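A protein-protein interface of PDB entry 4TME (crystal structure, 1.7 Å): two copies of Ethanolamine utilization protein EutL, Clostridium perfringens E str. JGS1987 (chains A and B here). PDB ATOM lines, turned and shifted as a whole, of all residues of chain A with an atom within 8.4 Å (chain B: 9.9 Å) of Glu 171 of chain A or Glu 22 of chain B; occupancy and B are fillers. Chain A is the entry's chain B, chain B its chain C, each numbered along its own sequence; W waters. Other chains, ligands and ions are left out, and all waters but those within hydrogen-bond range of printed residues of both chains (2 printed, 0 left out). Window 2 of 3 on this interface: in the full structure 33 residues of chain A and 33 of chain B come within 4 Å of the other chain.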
ATOM      1  N   ALA A 139       9.338 -21.210   9.195  1.00  0.00           N
ATOM      2  CA  ALA A 139       9.779 -20.945  10.560  1.00  0.00           C
ATOM      3  C   ALA A 139       9.312 -19.587  11.087  1.00  0.00           C
ATOM      4  O   ALA A 139       9.379 -19.319  12.279  1.00  0.00           O
ATOM      5  CB  ALA A 139      11.311 -21.028  10.640  1.00  0.00           C
ATOM      6  N   ILE A 141      10.825 -16.553  10.208  1.00  0.00           N
ATOM      7  CA  ILE A 141      12.012 -15.757  10.428  1.00  0.00           C
ATOM      8  C   ILE A 141      12.385 -15.039   9.122  1.00  0.00           C
ATOM      9  O   ILE A 141      11.869 -15.382   8.055  1.00  0.00           O
ATOM     10  CB  ILE A 141      13.199 -16.604  10.915  1.00  0.00           C
ATOM     11  CG1 ILE A 141      13.625 -17.618   9.852  1.00  0.00           C
ATOM     12  CG2 ILE A 141      12.815 -17.309  12.241  1.00  0.00           C
ATOM     13  CD1 ILE A 141      14.771 -18.561  10.324  1.00  0.00           C
ATOM     14  N   GLU A 145      18.257 -16.075   7.758  1.00  0.00           N
ATOM     15  CA  GLU A 145      18.616 -16.411   9.141  1.00  0.00           C
ATOM     16  C   GLU A 145      18.810 -17.909   9.278  1.00  0.00           C
ATOM     17  O   GLU A 145      18.455 -18.657   8.397  1.00  0.00           O
ATOM     18  CB  GLU A 145      17.584 -15.836  10.108  1.00  0.00           C
ATOM     19  CG  GLU A 145      18.005 -14.373  10.404  1.00  0.00           C
ATOM     20  CD  GLU A 145      17.007 -13.560  11.183  1.00  0.00           C
ATOM     21  OE1 GLU A 145      15.976 -14.112  11.621  1.00  0.00           O
ATOM     22  OE2 GLU A 145      17.258 -12.343  11.337  1.00  0.00           O
ATOM     23  N   ALA A 146      19.452 -18.334  10.371  1.00  0.00           N
ATOM     24  CA  ALA A 146      19.841 -19.745  10.527  1.00  0.00           C
ATOM     25  C   ALA A 146      18.774 -20.580  11.210  1.00  0.00           C
ATOM     26  O   ALA A 146      17.958 -20.045  11.966  1.00  0.00           O
ATOM     27  CB  ALA A 146      21.159 -19.828  11.329  1.00  0.00           C
ATOM     28  N   LEU A 147      18.778 -21.885  10.936  1.00  0.00           N
ATOM     29  CA  LEU A 147      17.915 -22.843  11.643  1.00  0.00           C
ATOM     30  C   LEU A 147      18.691 -24.073  12.076  1.00  0.00           C
ATOM     31  O   LEU A 147      19.651 -24.473  11.414  1.00  0.00           O
ATOM     32  CB  LEU A 147      16.751 -23.308  10.746  1.00  0.00           C
ATOM     33  CG  LEU A 147      15.642 -22.314  10.399  1.00  0.00           C
ATOM     34  CD1 LEU A 147      14.744 -22.942   9.335  1.00  0.00           C
ATOM     35  CD2 LEU A 147      14.844 -21.891  11.612  1.00  0.00           C
ATOM     36  N   ALA A 148      18.289 -24.646  13.213  1.00  0.00           N
ATOM     37  CA  ALA A 148      18.518 -26.057  13.501  1.00  0.00           C
ATOM     38  C   ALA A 148      17.266 -26.811  13.088  1.00  0.00           C
ATOM     39  O   ALA A 148      16.174 -26.512  13.574  1.00  0.00           O
ATOM     40  CB  ALA A 148      18.816 -26.277  14.972  1.00  0.00           C
ATOM     41  N   LEU A 161      14.636 -32.492  21.981  1.00  0.00           N
ATOM     42  CA  LEU A 161      14.342 -31.068  21.820  1.00  0.00           C
ATOM     43  C   LEU A 161      14.546 -30.321  23.120  1.00  0.00           C
ATOM     44  O   LEU A 161      15.105 -29.228  23.138  1.00  0.00           O
ATOM     45  CB  LEU A 161      12.910 -30.838  21.313  1.00  0.00           C
ATOM     46  CG  LEU A 161      12.653 -31.077  19.825  1.00  0.00           C
ATOM     47  CD1 LEU A 161      11.168 -30.907  19.555  1.00  0.00           C
ATOM     48  CD2 LEU A 161      13.477 -30.158  18.906  1.00  0.00           C
ATOM     49  N   ASP A 162      14.097 -30.908  24.224  1.00  0.00           N
ATOM     50  CA  ASP A 162      14.286 -30.264  25.504  1.00  0.00           C
ATOM     51  C   ASP A 162      15.773 -30.101  25.758  1.00  0.00           C
ATOM     52  O   ASP A 162      16.242 -29.041  26.183  1.00  0.00           O
ATOM     53  CB  ASP A 162      13.637 -31.078  26.619  1.00  0.00           C
ATOM     54  CG  ASP A 162      13.810 -30.406  27.973  1.00  0.00           C
ATOM     55  OD1 ASP A 162      13.160 -29.360  28.176  1.00  0.00           O
ATOM     56  OD2 ASP A 162      14.605 -30.888  28.787  1.00  0.00           O
ATOM     57  N   ALA A 164      18.156 -29.896  23.497  1.00  0.00           N
ATOM     58  CA  ALA A 164      18.694 -28.903  22.568  1.00  0.00           C
ATOM     59  C   ALA A 164      18.387 -27.479  23.043  1.00  0.00           C
ATOM     60  O   ALA A 164      19.252 -26.598  23.005  1.00  0.00           O
ATOM     61  CB  ALA A 164      18.133 -29.117  21.169  1.00  0.00           C
ATOM     62  N   LEU A 165      17.158 -27.256  23.513  1.00  0.00           N
ATOM     63  CA  LEU A 165      16.754 -25.932  23.984  1.00  0.00           C
ATOM     64  C   LEU A 165      17.530 -25.499  25.223  1.00  0.00           C
ATOM     65  O   LEU A 165      17.828 -24.313  25.392  1.00  0.00           O
ATOM     66  CB  LEU A 165      15.244 -25.899  24.279  1.00  0.00           C
ATOM     67  CG  LEU A 165      14.356 -25.989  23.046  1.00  0.00           C
ATOM     68  CD1 LEU A 165      12.962 -26.523  23.404  1.00  0.00           C
ATOM     69  CD2 LEU A 165      14.265 -24.609  22.399  1.00  0.00           C
ATOM     70  N   LYS A 166      17.860 -26.440  26.099  1.00  0.00           N
ATOM     71  CA  LYS A 166      18.610 -26.086  27.293  1.00  0.00           C
ATOM     72  C   LYS A 166      20.086 -25.854  26.977  1.00  0.00           C
ATOM     73  O   LYS A 166      20.734 -25.037  27.629  1.00  0.00           O
ATOM     74  CB  LYS A 166      18.447 -27.169  28.353  1.00  0.00           C
ATOM     75  CG  LYS A 166      17.040 -27.151  28.943  1.00  0.00           C
ATOM     76  CD  LYS A 166      16.777 -28.290  29.882  1.00  0.00           C
ATOM     77  CE  LYS A 166      15.363 -28.198  30.449  1.00  0.00           C
ATOM     78  NZ  LYS A 166      14.966 -29.466  31.082  1.00  0.00           N
ATOM     79  N   ALA A 168      21.551 -24.823  24.105  1.00  0.00           N
ATOM     80  CA  ALA A 168      21.913 -23.875  23.060  1.00  0.00           C
ATOM     81  C   ALA A 168      21.068 -22.616  23.112  1.00  0.00           C
ATOM     82  O   ALA A 168      19.917 -22.643  23.529  1.00  0.00           O
ATOM     83  CB  ALA A 168      21.780 -24.547  21.693  1.00  0.00           C
ATOM     84  N   ASP A 169      21.652 -21.521  22.644  1.00  0.00           N
ATOM     85  CA  ASP A 169      21.024 -20.213  22.702  1.00  0.00           C
ATOM     86  C   ASP A 169      20.101 -20.021  21.495  1.00  0.00           C
ATOM     87  O   ASP A 169      20.347 -19.176  20.613  1.00  0.00           O
ATOM     88  CB  ASP A 169      22.110 -19.135  22.774  1.00  0.00           C
ATOM     89  CG  ASP A 169      21.548 -17.762  23.068  1.00  0.00           C
ATOM     90  OD1 ASP A 169      20.380 -17.670  23.519  1.00  0.00           O
ATOM     91  OD2 ASP A 169      22.272 -16.778  22.864  1.00  0.00           O
ATOM     92  N   VAL A 170      19.028 -20.811  21.477  1.00  0.00           N
ATOM     93  CA  VAL A 170      18.094 -20.852  20.345  1.00  0.00           C
ATOM     94  C   VAL A 170      16.651 -20.617  20.796  1.00  0.00           C
ATOM     95  O   VAL A 170      16.324 -20.706  21.988  1.00  0.00           O
ATOM     96  CB  VAL A 170      18.158 -22.201  19.590  1.00  0.00           C
ATOM     97  CG1 VAL A 170      19.525 -22.380  18.930  1.00  0.00           C
ATOM     98  CG2 VAL A 170      17.805 -23.402  20.535  1.00  0.00           C
ATOM     99  N   GLU A 171      15.803 -20.304  19.825  1.00  0.00           N
ATOM    100  CA  GLU A 171      14.368 -20.090  20.028  1.00  0.00           C
ATOM    101  C   GLU A 171      13.558 -21.072  19.225  1.00  0.00           C
ATOM    102  O   GLU A 171      13.933 -21.429  18.109  1.00  0.00           O
ATOM    103  CB  GLU A 171      13.953 -18.689  19.593  1.00  0.00           C
ATOM    104  CG  GLU A 171      14.653 -17.551  20.289  1.00  0.00           C
ATOM    105  CD  GLU A 171      14.427 -16.260  19.541  1.00  0.00           C
ATOM    106  OE1 GLU A 171      15.308 -15.876  18.737  1.00  0.00           O
ATOM    107  OE2 GLU A 171      13.349 -15.656  19.732  1.00  0.00           O
ATOM    108  N   MET A 172      12.409 -21.460  19.763  1.00  0.00           N
ATOM    109  CA  MET A 172      11.470 -22.328  19.064  1.00  0.00           C
ATOM    110  C   MET A 172      10.744 -21.582  17.955  1.00  0.00           C
ATOM    111  O   MET A 172      10.234 -20.494  18.191  1.00  0.00           O
ATOM    112  CB  MET A 172      10.449 -22.878  20.068  1.00  0.00           C
ATOM    113  CG  MET A 172       9.248 -23.553  19.452  1.00  0.00           C
ATOM    114  SD  MET A 172       9.693 -25.041  18.600  1.00  0.00           S
ATOM    115  CE  MET A 172       9.959 -26.197  19.919  1.00  0.00           C
ATOM    116  N   CYS A 173      10.721 -22.148  16.756  1.00  0.00           N
ATOM    117  CA  CYS A 173       9.959 -21.550  15.655  1.00  0.00           C
ATOM    118  C   CYS A 173       8.751 -22.388  15.254  1.00  0.00           C
ATOM    119  O   CYS A 173       7.613 -21.922  15.306  1.00  0.00           O
ATOM    120  CB  CYS A 173      10.856 -21.356  14.438  1.00  0.00           C
ATOM    121  SG  CYS A 173      12.168 -20.180  14.732  1.00  0.00           S
ATOM    122  N   GLU A 174       9.014 -23.591  14.776  1.00  0.00           N
ATOM    123  CA  GLU A 174       7.964 -24.479  14.306  1.00  0.00           C
ATOM    124  C   GLU A 174       8.118 -25.832  14.989  1.00  0.00           C
ATOM    125  O   GLU A 174       9.204 -26.410  14.996  1.00  0.00           O
ATOM    126  CB  GLU A 174       8.037 -24.618  12.794  1.00  0.00           C
ATOM    127  CG  GLU A 174       6.929 -25.493  12.181  1.00  0.00           C
ATOM    128  CD  GLU A 174       5.586 -24.762  12.045  1.00  0.00           C
ATOM    129  OE1 GLU A 174       5.181 -24.008  12.963  1.00  0.00           O
ATOM    130  OE2 GLU A 174       4.932 -24.943  10.991  1.00  0.00           O
ATOM    131  N   PHE A 175       7.033 -26.313  15.583  1.00  0.00           N
ATOM    132  CA  PHE A 175       7.015 -27.586  16.289  1.00  0.00           C
ATOM    133  C   PHE A 175       6.357 -28.617  15.383  1.00  0.00           C
ATOM    134  O   PHE A 175       5.232 -28.402  14.909  1.00  0.00           O
ATOM    135  CB  PHE A 175       6.264 -27.434  17.609  1.00  0.00           C
ATOM    136  CG  PHE A 175       6.113 -28.716  18.402  1.00  0.00           C
ATOM    137  CD1 PHE A 175       7.211 -29.508  18.717  1.00  0.00           C
ATOM    138  CD2 PHE A 175       4.863 -29.096  18.877  1.00  0.00           C
ATOM    139  CE1 PHE A 175       7.048 -30.687  19.465  1.00  0.00           C
ATOM    140  CE2 PHE A 175       4.687 -30.254  19.629  1.00  0.00           C
ATOM    141  CZ  PHE A 175       5.770 -31.048  19.936  1.00  0.00           C
ATOM    142  N   ALA A 187      11.523 -30.148  15.483  1.00  0.00           N
ATOM    143  CA  ALA A 187      11.272 -28.700  15.414  1.00  0.00           C
ATOM    144  C   ALA A 187      12.254 -28.005  14.508  1.00  0.00           C
ATOM    145  O   ALA A 187      13.320 -28.539  14.194  1.00  0.00           O
ATOM    146  CB  ALA A 187      11.327 -28.061  16.813  1.00  0.00           C
ATOM    147  N   LEU A 188      11.878 -26.799  14.099  1.00  0.00           N
ATOM    148  CA  LEU A 188      12.813 -25.810  13.601  1.00  0.00           C
ATOM    149  C   LEU A 188      13.094 -24.810  14.706  1.00  0.00           C
ATOM    150  O   LEU A 188      12.156 -24.181  15.214  1.00  0.00           O
ATOM    151  CB  LEU A 188      12.243 -25.059  12.393  1.00  0.00           C
ATOM    152  CG  LEU A 188      11.777 -25.903  11.228  1.00  0.00           C
ATOM    153  CD1 LEU A 188      11.187 -24.973  10.136  1.00  0.00           C
ATOM    154  CD2 LEU A 188      12.921 -26.739  10.689  1.00  0.00           C
ATOM    155  N   LEU A 189      14.368 -24.683  15.076  1.00  0.00           N
ATOM    156  CA  LEU A 189      14.829 -23.720  16.078  1.00  0.00           C
ATOM    157  C   LEU A 189      15.713 -22.684  15.380  1.00  0.00           C
ATOM    158  O   LEU A 189      16.384 -23.010  14.413  1.00  0.00           O
ATOM    159  CB  LEU A 189      15.624 -24.395  17.211  1.00  0.00           C
ATOM    160  CG  LEU A 189      15.018 -25.663  17.832  1.00  0.00           C
ATOM    161  CD1 LEU A 189      15.901 -26.169  18.991  1.00  0.00           C
ATOM    162  CD2 LEU A 189      13.617 -25.428  18.323  1.00  0.00           C
ATOM    163  N   THR A 190      15.712 -21.449  15.856  1.00  0.00           N
ATOM    164  CA  THR A 190      16.545 -20.416  15.244  1.00  0.00           C
ATOM    165  C   THR A 190      17.475 -19.751  16.251  1.00  0.00           C
ATOM    166  O   THR A 190      17.267 -19.792  17.466  1.00  0.00           O
ATOM    167  CB  THR A 190      15.683 -19.323  14.508  1.00  0.00           C
ATOM    168  OG1 THR A 190      16.525 -18.496  13.685  1.00  0.00           O
ATOM    169  CG2 THR A 190      14.951 -18.428  15.475  1.00  0.00           C
ATOM    170  N   GLY A 191      18.532 -19.159  15.713  1.00  0.00           N
ATOM    171  CA  GLY A 191      19.539 -18.484  16.509  1.00  0.00           C
ATOM    172  C   GLY A 191      20.735 -18.163  15.624  1.00  0.00           C
ATOM    173  O   GLY A 191      20.613 -18.224  14.392  1.00  0.00           O
ATOM    174  N   SER A 192      21.872 -17.824  16.232  1.00  0.00           N
ATOM    175  CA  SER A 192      23.125 -17.683  15.478  1.00  0.00           C
ATOM    176  C   SER A 192      23.448 -19.027  14.838  1.00  0.00           C
ATOM    177  O   SER A 192      22.899 -20.065  15.257  1.00  0.00           O
ATOM    178  CB  SER A 192      24.264 -17.269  16.375  1.00  0.00           C
ATOM    179  OG  SER A 192      24.549 -18.302  17.308  1.00  0.00           O
ATOM    180  N   ALA A 195      24.808 -21.176  17.606  1.00  0.00           N
ATOM    181  CA  ALA A 195      23.799 -21.727  18.520  1.00  0.00           C
ATOM    182  C   ALA A 195      23.000 -22.842  17.851  1.00  0.00           C
ATOM    183  O   ALA A 195      22.642 -23.830  18.486  1.00  0.00           O
ATOM    184  CB  ALA A 195      22.866 -20.625  19.014  1.00  0.00           C
ATOM    185  N   CYS A 196      22.703 -22.682  16.565  1.00  0.00           N
ATOM    186  CA  CYS A 196      21.984 -23.718  15.840  1.00  0.00           C
ATOM    187  C   CYS A 196      22.825 -24.994  15.780  1.00  0.00           C
ATOM    188  O   CYS A 196      22.320 -26.090  15.972  1.00  0.00           O
ATOM    189  CB  CYS A 196      21.612 -23.237  14.447  1.00  0.00           C
ATOM    190  SG  CYS A 196      20.251 -22.052  14.510  1.00  0.00           S
ATOM    191  N   ALA A 199      22.731 -26.635  19.135  1.00  0.00           N
ATOM    192  CA  ALA A 199      21.447 -27.318  19.290  1.00  0.00           C
ATOM    193  C   ALA A 199      21.474 -28.663  18.556  1.00  0.00           C
ATOM    194  O   ALA A 199      21.007 -29.679  19.078  1.00  0.00           O
ATOM    195  CB  ALA A 199      20.315 -26.449  18.773  1.00  0.00           C
ATOM    196  N   ASN B  18      11.941 -29.935  34.689  1.00  0.00           N
ATOM    197  CA  ASN B  18      12.070 -28.506  34.449  1.00  0.00           C
ATOM    198  C   ASN B  18      11.941 -28.225  32.957  1.00  0.00           C
ATOM    199  O   ASN B  18      12.882 -27.773  32.307  1.00  0.00           O
ATOM    200  CB  ASN B  18      13.404 -28.002  34.989  1.00  0.00           C
ATOM    201  CG  ASN B  18      13.611 -28.373  36.455  1.00  0.00           C
ATOM    202  OD1 ASN B  18      12.735 -28.148  37.295  1.00  0.00           O
ATOM    203  ND2 ASN B  18      14.768 -28.962  36.765  1.00  0.00           N
ATOM    204  N   VAL B  19      10.768 -28.539  32.426  1.00  0.00           N
ATOM    205  CA  VAL B  19      10.523 -28.423  31.004  1.00  0.00           C
ATOM    206  C   VAL B  19      10.798 -26.986  30.552  1.00  0.00           C
ATOM    207  O   VAL B  19      10.467 -26.017  31.240  1.00  0.00           O
ATOM    208  CB  VAL B  19       9.069 -28.847  30.647  1.00  0.00           C
ATOM    209  CG1 VAL B  19       8.058 -27.927  31.300  1.00  0.00           C
ATOM    210  CG2 VAL B  19       8.883 -28.871  29.147  1.00  0.00           C
ATOM    211  N   SER B  20      11.449 -26.851  29.402  1.00  0.00           N
ATOM    212  CA  SER B  20      11.760 -25.544  28.882  1.00  0.00           C
ATOM    213  C   SER B  20      10.479 -24.778  28.576  1.00  0.00           C
ATOM    214  O   SER B  20       9.499 -25.371  28.126  1.00  0.00           O
ATOM    215  CB  SER B  20      12.605 -25.680  27.627  1.00  0.00           C
ATOM    216  OG  SER B  20      11.913 -26.443  26.663  1.00  0.00           O
ATOM    217  N   PRO B  21      10.485 -23.458  28.786  1.00  0.00           N
ATOM    218  CA  PRO B  21       9.313 -22.639  28.469  1.00  0.00           C
ATOM    219  C   PRO B  21       8.889 -22.717  26.999  1.00  0.00           C
ATOM    220  O   PRO B  21       7.702 -22.642  26.686  1.00  0.00           O
ATOM    221  CB  PRO B  21       9.774 -21.217  28.799  1.00  0.00           C
ATOM    222  CG  PRO B  21      10.864 -21.370  29.755  1.00  0.00           C
ATOM    223  CD  PRO B  21      11.549 -22.662  29.437  1.00  0.00           C
ATOM    224  N   GLU B  22       9.862 -22.835  26.102  1.00  0.00           N
ATOM    225  CA  GLU B  22       9.570 -22.877  24.675  1.00  0.00           C
ATOM    226  C   GLU B  22       8.766 -24.129  24.327  1.00  0.00           C
ATOM    227  O   GLU B  22       7.863 -24.090  23.485  1.00  0.00           O
ATOM    228  CB  GLU B  22      10.865 -22.821  23.859  1.00  0.00           C
ATOM    229  CG  GLU B  22      11.535 -21.445  23.813  1.00  0.00           C
ATOM    230  CD  GLU B  22      10.857 -20.466  22.846  1.00  0.00           C
ATOM    231  OE1 GLU B  22      11.568 -19.875  21.999  1.00  0.00           O
ATOM    232  OE2 GLU B  22       9.620 -20.276  22.937  1.00  0.00           O
ATOM    233  N   MET B  23       9.078 -25.239  24.983  1.00  0.00           N
ATOM    234  CA  MET B  23       8.311 -26.462  24.793  1.00  0.00           C
ATOM    235  C   MET B  23       6.973 -26.417  25.525  1.00  0.00           C
ATOM    236  O   MET B  23       5.961 -26.867  24.987  1.00  0.00           O
ATOM    237  CB  MET B  23       9.102 -27.665  25.271  1.00  0.00           C
ATOM    238  CG  MET B  23       8.368 -28.969  25.099  1.00  0.00           C
ATOM    239  SD  MET B  23       9.351 -30.386  25.610  1.00  0.00           S
ATOM    240  CE  MET B  23      10.728 -30.220  24.509  1.00  0.00           C
ATOM    241  N   ALA B  24       6.976 -25.862  26.736  1.00  0.00           N
ATOM    242  CA  ALA B  24       5.757 -25.734  27.526  1.00  0.00           C
ATOM    243  C   ALA B  24       4.700 -25.019  26.697  1.00  0.00           C
ATOM    244  O   ALA B  24       3.535 -25.434  26.680  1.00  0.00           O
ATOM    245  CB  ALA B  24       6.029 -24.988  28.835  1.00  0.00           C
ATOM    246  N   LYS B  25       5.110 -23.982  25.966  1.00  0.00           N
ATOM    247  CA  LYS B  25       4.183 -23.219  25.140  1.00  0.00           C
ATOM    248  C   LYS B  25       3.626 -24.034  23.974  1.00  0.00           C
ATOM    249  O   LYS B  25       2.420 -23.959  23.678  1.00  0.00           O
ATOM    250  CB  LYS B  25       4.858 -21.953  24.590  1.00  0.00           C
ATOM    251  CG  LYS B  25       4.489 -20.683  25.349  1.00  0.00           C
ATOM    252  CD  LYS B  25       5.149 -19.431  24.753  1.00  0.00           C
ATOM    253  CE  LYS B  25       6.587 -19.250  25.241  1.00  0.00           C
ATOM    254  NZ  LYS B  25       6.701 -18.990  26.718  1.00  0.00           N
ATOM    255  N   LYS B  26       4.483 -24.805  23.304  1.00  0.00           N
ATOM    256  CA  LYS B  26       4.017 -25.574  22.154  1.00  0.00           C
ATOM    257  C   LYS B  26       3.109 -26.731  22.574  1.00  0.00           C
ATOM    258  O   LYS B  26       2.254 -27.174  21.794  1.00  0.00           O
ATOM    259  CB  LYS B  26       5.201 -26.096  21.326  1.00  0.00           C
ATOM    260  CG  LYS B  26       5.953 -24.998  20.574  1.00  0.00           C
ATOM    261  CD  LYS B  26       5.099 -24.361  19.464  1.00  0.00           C
ATOM    262  CE  LYS B  26       5.890 -23.343  18.664  1.00  0.00           C
ATOM    263  NZ  LYS B  26       5.048 -22.710  17.602  1.00  0.00           N
ATOM    264  N   LEU B  27       3.286 -27.213  23.798  1.00  0.00           N
ATOM    265  CA  LEU B  27       2.434 -28.277  24.332  1.00  0.00           C
ATOM    266  C   LEU B  27       1.215 -27.723  25.088  1.00  0.00           C
ATOM    267  O   LEU B  27       0.392 -28.490  25.585  1.00  0.00           O
ATOM    268  CB  LEU B  27       3.242 -29.182  25.259  1.00  0.00           C
ATOM    269  CG  LEU B  27       4.315 -30.032  24.593  1.00  0.00           C
ATOM    270  CD1 LEU B  27       5.134 -30.768  25.650  1.00  0.00           C
ATOM    271  CD2 LEU B  27       3.684 -31.021  23.598  1.00  0.00           C
ATOM    272  N   GLU B  28       1.116 -26.400  25.167  1.00  0.00           N
ATOM    273  CA  GLU B  28      -0.002 -25.731  25.827  1.00  0.00           C
ATOM    274  C   GLU B  28      -0.182 -26.191  27.279  1.00  0.00           C
ATOM    275  O   GLU B  28      -1.303 -26.427  27.747  1.00  0.00           O
ATOM    276  CB  GLU B  28      -1.293 -25.957  25.026  1.00  0.00           C
ATOM    277  CG  GLU B  28      -1.189 -25.456  23.594  1.00  0.00           C
ATOM    278  CD  GLU B  28      -2.488 -25.559  22.813  1.00  0.00           C
ATOM    279  OE1 GLU B  28      -3.252 -26.525  23.012  1.00  0.00           O
ATOM    280  OE2 GLU B  28      -2.732 -24.668  21.982  1.00  0.00           O
ATOM    281  N   LEU B  29       0.935 -26.300  27.985  1.00  0.00           N
ATOM    282  CA  LEU B  29       0.935 -26.727  29.378  1.00  0.00           C
ATOM    283  C   LEU B  29       0.391 -25.656  30.308  1.00  0.00           C
ATOM    284  O   LEU B  29       0.472 -24.451  30.012  1.00  0.00           O
ATOM    285  CB  LEU B  29       2.344 -27.083  29.821  1.00  0.00           C
ATOM    286  CG  LEU B  29       3.065 -28.173  29.031  1.00  0.00           C
ATOM    287  CD1 LEU B  29       4.426 -28.382  29.651  1.00  0.00           C
ATOM    288  CD2 LEU B  29       2.260 -29.461  29.038  1.00  0.00           C
ATOM    289  N   LEU B  36       7.694 -33.457  32.744  1.00  0.00           N
ATOM    290  CA  LEU B  36       6.967 -34.337  31.823  1.00  0.00           C
ATOM    291  C   LEU B  36       7.445 -35.778  31.913  1.00  0.00           C
ATOM    292  O   LEU B  36       8.630 -36.029  32.079  1.00  0.00           O
ATOM    293  CB  LEU B  36       7.129 -33.869  30.371  1.00  0.00           C
ATOM    294  CG  LEU B  36       6.758 -32.415  30.059  1.00  0.00           C
ATOM    295  CD1 LEU B  36       7.062 -32.155  28.571  1.00  0.00           C
ATOM    296  CD2 LEU B  36       5.314 -32.130  30.384  1.00  0.00           C
HETATM  297  O   HOH W   1       6.513 -20.026  16.875  1.00  0.00           O
HETATM  298  O   HOH W   2       4.642 -24.734  15.634  1.00  0.00           O
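No position is printed for both chains. Of the 11 pairs that touch across the chains among the printed residues, none has its exchanged pair printed and touching as well.
Among the printed residues, pairs that only touch across the chains: Leu 165 of chain A with Ser 20 of chain B (3.4 Å), Glu 171 of chain A with Glu 22 of chain B (3.4 Å), Asp 162 of chain A with Met 23 of chain B (3.5 Å), Met 172 of chain A with Lys 26 of chain B (3.5 Å), Cys 173 of chain A with Lys 26 of chain B (3.5 Å), Phe 175 of chain A with Lys 26 of chain B (3.8 Å), Leu 161 of chain A with Met 23 of chain B (3.9 Å) and Asp 162 of chain A with Val 19 of chain B (3.98 Å).
Of the printed residues of chain B, Leu 161 of chain A touches Met 23. Printed residues of chain B within 4 Å of Lys 166 of chain A: Asn 18 (3.0 Å). Printed residues of chain B within 4 Å of Glu 171 of chain A: Glu 22 (3.4 Å). Printed residues of chain B within 4 Å of Phe 175 of chain A: Lys 26 (3.8 Å). No residue of chain B comes within 4 Å of Leu 189 of chain A. Thr 190 of chain A touches none of the printed residues of chain B. Ala 199 of chain A touches none of the printed residues of chain B. Pro 21 of chain B touches none of the printed residues of chain A. Of the printed residues of chain A, Glu 22 of chain B touches Glu 171 and Met 172. Lys 25 of chain B touches none of the printed residues of chain A. The nearest printed residue of chain A that does not touch Glu 22 of chain B is Leu 165 of chain A (4.1 Å).
The backbone NH (N) of Met 172 of chain A is in hydrogen-bond range of the side-chain carboxylate (OE1) of Glu 22 of chain B (2.9 Å). The backbone carbonyl oxygen of Asn 18 of chain B lies within hydrogen-bond range of the side-chain amino group of Lys 166 of chain A, 3.0 Å away. The backbone NH (N) of Ser 20 of chain B is in hydrogen-bond range of the side-chain carboxylate (OD1) of Asp 162 of chain A.
Of the 28 printed residues of chain A, 8 touch a printed residue of chain B. Printed residues of chain A that touch a printed residue of chain B: Leu 161, Asp 162, Leu 165, Lys 166, Glu 171, Met 172, Cys 173 and Phe 175. Hydrophobic or aromatic side chains of chain A within 4 Å of the printed part of chain B: Leu 161, Leu 165, Met 172 and Phe 175. Along chain A the printed residues that touch a printed residue of chain B span positions 161 to 175. Of the 13 printed residues of chain B, 6 touch a printed residue of chain A. Among the printed residues, no Asp or Glu carboxylate lies within 4 Å of a Lys or Arg side-chain nitrogen of the other chain.
OD2 of Asp 162 of chain A is in salt-bridge range of NZ of Lys 166 of chain A. The backbone NH (N) of Glu 171 of chain A sits at hydrogen-bond distance from the backbone carbonyl oxygen (O) of Thr 190 of chain A (2.8 Å). O of Leu 188 of chain A lies within hydrogen-bond range of N of Cys 173 of chain A, at 2.9 Å.
Water W1 lies within hydrogen-bond range of the backbone carbonyl oxygen of Cys 173 of chain A (2.7 Å) and the side-chain amino group of Lys 26 of chain B (3.1 Å). Water W2 lies within hydrogen-bond range of OE1 of Glu 174 of chain A, NZ of Lys 26 of chain B and N of Phe 175 of chain A.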
